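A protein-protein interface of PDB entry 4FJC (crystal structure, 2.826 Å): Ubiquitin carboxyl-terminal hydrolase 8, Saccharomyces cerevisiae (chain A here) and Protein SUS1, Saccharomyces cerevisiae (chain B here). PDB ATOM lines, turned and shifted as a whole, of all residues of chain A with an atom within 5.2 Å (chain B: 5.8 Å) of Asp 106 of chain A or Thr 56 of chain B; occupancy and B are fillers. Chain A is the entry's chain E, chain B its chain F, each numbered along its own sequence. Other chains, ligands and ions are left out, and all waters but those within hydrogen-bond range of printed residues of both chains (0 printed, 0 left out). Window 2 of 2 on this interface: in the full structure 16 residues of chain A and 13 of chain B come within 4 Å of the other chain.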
ATOM      1  N   LEU A  99      25.167  24.455 -22.346  1.00  0.00           N
ATOM      2  CA  LEU A  99      26.091  24.991 -21.350  1.00  0.00           C
ATOM      3  C   LEU A  99      26.540  23.910 -20.380  1.00  0.00           C
ATOM      4  O   LEU A  99      25.728  23.285 -19.704  1.00  0.00           O
ATOM      5  CB  LEU A  99      25.450  26.135 -20.552  1.00  0.00           C
ATOM      6  CG  LEU A  99      26.367  26.782 -19.491  1.00  0.00           C
ATOM      7  CD1 LEU A  99      27.575  27.465 -20.111  1.00  0.00           C
ATOM      8  CD2 LEU A  99      25.590  27.768 -18.644  1.00  0.00           C
ATOM      9  N   PHE A 100      27.851  23.767 -20.264  1.00  0.00           N
ATOM     10  CA  PHE A 100      28.448  22.636 -19.615  1.00  0.00           C
ATOM     11  C   PHE A 100      29.190  23.145 -18.411  1.00  0.00           C
ATOM     12  O   PHE A 100      29.896  24.142 -18.528  1.00  0.00           O
ATOM     13  CB  PHE A 100      29.423  21.983 -20.591  1.00  0.00           C
ATOM     14  CG  PHE A 100      29.915  20.640 -20.153  1.00  0.00           C
ATOM     15  CD1 PHE A 100      29.092  19.536 -20.229  1.00  0.00           C
ATOM     16  CD2 PHE A 100      31.211  20.471 -19.701  1.00  0.00           C
ATOM     17  CE1 PHE A 100      29.529  18.286 -19.844  1.00  0.00           C
ATOM     18  CE2 PHE A 100      31.656  19.222 -19.316  1.00  0.00           C
ATOM     19  CZ  PHE A 100      30.808  18.128 -19.380  1.00  0.00           C
ATOM     20  N   CYS A 101      29.024  22.477 -17.266  1.00  0.00           N
ATOM     21  CA  CYS A 101      29.852  22.756 -16.089  1.00  0.00           C
ATOM     22  C   CYS A 101      30.939  21.718 -15.996  1.00  0.00           C
ATOM     23  O   CYS A 101      30.663  20.531 -15.939  1.00  0.00           O
ATOM     24  CB  CYS A 101      29.080  22.741 -14.781  1.00  0.00           C
ATOM     25  SG  CYS A 101      30.231  22.720 -13.370  1.00  0.00           S
ATOM     26  N   CYS A 104      31.171  19.849 -12.415  1.00  0.00           N
ATOM     27  CA  CYS A 104      30.186  18.762 -12.396  1.00  0.00           C
ATOM     28  C   CYS A 104      30.476  17.682 -13.445  1.00  0.00           C
ATOM     29  O   CYS A 104      30.123  16.530 -13.244  1.00  0.00           O
ATOM     30  CB  CYS A 104      28.771  19.287 -12.647  1.00  0.00           C
ATOM     31  SG  CYS A 104      28.103  20.379 -11.378  1.00  0.00           S
ATOM     32  N   GLU A 105      31.093  18.068 -14.566  1.00  0.00           N
ATOM     33  CA  GLU A 105      31.307  17.195 -15.750  1.00  0.00           C
ATOM     34  C   GLU A 105      30.014  16.733 -16.426  1.00  0.00           C
ATOM     35  O   GLU A 105      29.920  15.602 -16.909  1.00  0.00           O
ATOM     36  CB  GLU A 105      32.203  16.005 -15.415  1.00  0.00           C
ATOM     37  CG  GLU A 105      33.484  16.406 -14.703  1.00  0.00           C
ATOM     38  CD  GLU A 105      34.537  15.314 -14.728  1.00  0.00           C
ATOM     39  OE1 GLU A 105      34.169  14.124 -14.684  1.00  0.00           O
ATOM     40  OE2 GLU A 105      35.741  15.646 -14.801  1.00  0.00           O
ATOM     41  N   ASP A 106      29.045  17.648 -16.491  1.00  0.00           N
ATOM     42  CA  ASP A 106      27.716  17.387 -17.048  1.00  0.00           C
ATOM     43  C   ASP A 106      27.186  18.705 -17.618  1.00  0.00           C
ATOM     44  O   ASP A 106      27.713  19.770 -17.291  1.00  0.00           O
ATOM     45  CB  ASP A 106      26.809  16.894 -15.924  1.00  0.00           C
ATOM     46  CG  ASP A 106      25.569  16.180 -16.416  1.00  0.00           C
ATOM     47  OD1 ASP A 106      25.043  16.487 -17.509  1.00  0.00           O
ATOM     48  OD2 ASP A 106      25.096  15.300 -15.676  1.00  0.00           O
ATOM     49  N   TYR A 107      26.187  18.644 -18.494  1.00  0.00           N
ATOM     50  CA  TYR A 107      25.594  19.868 -19.045  1.00  0.00           C
ATOM     51  C   TYR A 107      24.557  20.419 -18.060  1.00  0.00           C
ATOM     52  O   TYR A 107      23.871  19.658 -17.384  1.00  0.00           O
ATOM     53  CB  TYR A 107      24.961  19.639 -20.438  1.00  0.00           C
ATOM     54  CG  TYR A 107      25.940  19.565 -21.604  1.00  0.00           C
ATOM     55  CD1 TYR A 107      26.306  20.700 -22.310  1.00  0.00           C
ATOM     56  CD2 TYR A 107      26.484  18.350 -22.005  1.00  0.00           C
ATOM     57  CE1 TYR A 107      27.203  20.629 -23.374  1.00  0.00           C
ATOM     58  CE2 TYR A 107      27.376  18.263 -23.059  1.00  0.00           C
ATOM     59  CZ  TYR A 107      27.747  19.401 -23.749  1.00  0.00           C
ATOM     60  OH  TYR A 107      28.650  19.300 -24.816  1.00  0.00           O
ATOM     61  N   ILE A 108      24.454  21.740 -17.964  1.00  0.00           N
ATOM     62  CA  ILE A 108      23.412  22.336 -17.137  1.00  0.00           C
ATOM     63  C   ILE A 108      22.131  22.252 -17.954  1.00  0.00           C
ATOM     64  O   ILE A 108      21.833  23.134 -18.753  1.00  0.00           O
ATOM     65  CB  ILE A 108      23.728  23.789 -16.682  1.00  0.00           C
ATOM     66  CG1 ILE A 108      24.967  23.813 -15.778  1.00  0.00           C
ATOM     67  CG2 ILE A 108      22.561  24.371 -15.890  1.00  0.00           C
ATOM     68  CD1 ILE A 108      25.682  25.149 -15.755  1.00  0.00           C
ATOM     69  N   MET B  50      21.399   5.441 -20.558  1.00  0.00           N
ATOM     70  CA  MET B  50      20.801   6.243 -19.479  1.00  0.00           C
ATOM     71  C   MET B  50      19.870   5.432 -18.561  1.00  0.00           C
ATOM     72  O   MET B  50      19.683   5.810 -17.412  1.00  0.00           O
ATOM     73  CB  MET B  50      20.031   7.443 -20.027  1.00  0.00           C
ATOM     74  CG  MET B  50      20.905   8.582 -20.517  1.00  0.00           C
ATOM     75  SD  MET B  50      19.999  10.117 -20.866  1.00  0.00           S
ATOM     76  CE  MET B  50      18.998   9.655 -22.280  1.00  0.00           C
ATOM     77  N   GLU B  54      20.939   3.900 -15.097  1.00  0.00           N
ATOM     78  CA  GLU B  54      20.051   4.751 -14.287  1.00  0.00           C
ATOM     79  C   GLU B  54      20.466   6.234 -14.153  1.00  0.00           C
ATOM     80  O   GLU B  54      19.939   6.921 -13.287  1.00  0.00           O
ATOM     81  CB  GLU B  54      19.888   4.130 -12.886  1.00  0.00           C
ATOM     82  CG  GLU B  54      19.699   2.609 -12.900  1.00  0.00           C
ATOM     83  CD  GLU B  54      19.053   2.037 -11.637  1.00  0.00           C
ATOM     84  OE1 GLU B  54      19.568   2.260 -10.517  1.00  0.00           O
ATOM     85  OE2 GLU B  54      18.029   1.335 -11.771  1.00  0.00           O
ATOM     86  N   SER B  55      21.361   6.725 -15.024  1.00  0.00           N
ATOM     87  CA  SER B  55      21.968   8.080 -14.912  1.00  0.00           C
ATOM     88  C   SER B  55      21.844   8.929 -16.183  1.00  0.00           C
ATOM     89  O   SER B  55      21.567   8.398 -17.263  1.00  0.00           O
ATOM     90  CB  SER B  55      23.463   7.980 -14.559  1.00  0.00           C
ATOM     91  OG  SER B  55      24.084   9.263 -14.540  1.00  0.00           O
ATOM     92  N   THR B  56      22.075  10.241 -16.032  1.00  0.00           N
ATOM     93  CA  THR B  56      22.028  11.203 -17.142  1.00  0.00           C
ATOM     94  C   THR B  56      23.244  12.155 -17.140  1.00  0.00           C
ATOM     95  O   THR B  56      23.155  13.326 -17.573  1.00  0.00           O
ATOM     96  CB  THR B  56      20.744  12.054 -17.092  1.00  0.00           C
ATOM     97  OG1 THR B  56      20.852  13.041 -16.056  1.00  0.00           O
ATOM     98  CG2 THR B  56      19.511  11.178 -16.858  1.00  0.00           C
ATOM     99  N   ASN B  57      24.380  11.660 -16.654  1.00  0.00           N
ATOM    100  CA  ASN B  57      25.599  12.453 -16.624  1.00  0.00           C
ATOM    101  C   ASN B  57      26.304  12.341 -17.954  1.00  0.00           C
ATOM    102  O   ASN B  57      26.719  11.252 -18.349  1.00  0.00           O
ATOM    103  CB  ASN B  57      26.526  12.009 -15.491  1.00  0.00           C
ATOM    104  CG  ASN B  57      27.807  12.815 -15.445  1.00  0.00           C
ATOM    105  OD1 ASN B  57      28.745  12.570 -16.212  1.00  0.00           O
ATOM    106  ND2 ASN B  57      27.850  13.797 -14.555  1.00  0.00           N
ATOM    107  N   PHE B  58      26.459  13.475 -18.631  1.00  0.00           N
ATOM    108  CA  PHE B  58      27.010  13.486 -19.975  1.00  0.00           C
ATOM    109  C   PHE B  58      28.333  12.780 -20.140  1.00  0.00           C
ATOM    110  O   PHE B  58      28.529  12.080 -21.124  1.00  0.00           O
ATOM    111  CB  PHE B  58      27.238  14.889 -20.480  1.00  0.00           C
ATOM    112  CG  PHE B  58      27.946  14.909 -21.798  1.00  0.00           C
ATOM    113  CD1 PHE B  58      27.236  14.751 -22.976  1.00  0.00           C
ATOM    114  CD2 PHE B  58      29.318  15.010 -21.859  1.00  0.00           C
ATOM    115  CE1 PHE B  58      27.880  14.737 -24.194  1.00  0.00           C
ATOM    116  CE2 PHE B  58      29.970  14.997 -23.068  1.00  0.00           C
ATOM    117  CZ  PHE B  58      29.247  14.861 -24.238  1.00  0.00           C
ATOM    118  N   THR B  59      29.260  13.029 -19.214  1.00  0.00           N
ATOM    119  CA  THR B  59      30.611  12.442 -19.270  1.00  0.00           C
ATOM    120  C   THR B  59      30.557  10.923 -19.220  1.00  0.00           C
ATOM    121  O   THR B  59      31.245  10.240 -19.982  1.00  0.00           O
ATOM    122  CB  THR B  59      31.505  12.968 -18.122  1.00  0.00           C
ATOM    123  OG1 THR B  59      31.788  14.365 -18.331  1.00  0.00           O
ATOM    124  CG2 THR B  59      32.803  12.196 -18.065  1.00  0.00           C
ATOM    125  N   ILE B  61      27.730   8.771 -19.659  1.00  0.00           N
ATOM    126  CA  ILE B  61      27.009   8.175 -20.786  1.00  0.00           C
ATOM    127  C   ILE B  61      27.914   8.163 -22.032  1.00  0.00           C
ATOM    128  O   ILE B  61      27.938   7.193 -22.786  1.00  0.00           O
ATOM    129  CB  ILE B  61      25.686   8.917 -21.099  1.00  0.00           C
ATOM    130  CG1 ILE B  61      24.755   9.011 -19.868  1.00  0.00           C
ATOM    131  CG2 ILE B  61      24.967   8.250 -22.253  1.00  0.00           C
ATOM    132  CD1 ILE B  61      24.508   7.726 -19.112  1.00  0.00           C
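Asp 106 of chain A touches just these residues of chain B: Thr 56, Asn 57 and Phe 58.
Of chain A, only Asp 106 (3.4 Å) comes within 4 Å of Thr 56 of chain B.
Of the printed residues of chain A, Asn 57 of chain B touches Cys 104 (3.8 Å), Glu 105 (3.3 Å) and Asp 106 (3.0 Å).
Printed residues of chain B within 4 Å of Cys 104 of chain A: Asn 57.
The nearest residue of chain B that does not touch Asp 106 of chain A is Thr 59 of chain B (4.7 Å).
The nearest printed residue of chain B that does not touch Glu 105 of chain A is Phe 58 of chain B (4.4 Å).
The side-chain amide oxygen of Asn 57 of chain B lies close to the backbone carbonyl oxygen of Glu 105 of chain A, at 3.3 Å.
ND2 of Asn 57 of chain B sits close to OD2 of Asp 106 of chain A, at 3.3 Å.
O of Thr 56 of chain B sits close to OD2 of Asp 106 of chain A (3.4 Å).
O of Glu 105 of chain A is in hydrogen-bond range of OG1 of Thr 59 of chain B (2.7 Å).
The backbone NH (N) of Asn 57 of chain B sits at hydrogen-bond distance from the side-chain hydroxyl (OG) of Ser 55 of chain B, at 3.2 Å.
The backbone carbonyl oxygen (O) of Asp 106 of chain A sits at hydrogen-bond distance from the backbone NH (N) of Cys 101 of chain A, at 3.0 Å.
OD1 of Asn 57 of chain B is in hydrogen-bond range of N of Thr 59 of chain B (3.1 Å).
Among the printed residues, merely in contact across the chains: Asp 106 of chain A with Phe 58 of chain B (3.5 Å), Tyr 107 of chain A with Phe 58 of chain B (3.5 Å), Cys 104 of chain A with Asn 57 of chain B (3.8 Å) and Phe 100 of chain A with Phe 58 of chain B (3.9 Å).
Of the 8 printed residues of chain A, 5 touch a printed residue of chain B.
Hydrophobic or aromatic side chains of chain A within 4 Å of the printed part of chain B: Phe 100 and Tyr 107.
Printed residues of chain B that touch a printed residue of chain A: Thr 56, Asn 57, Phe 58 and Thr 59.
Among the printed residues, 8 pairs touch across the chains.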
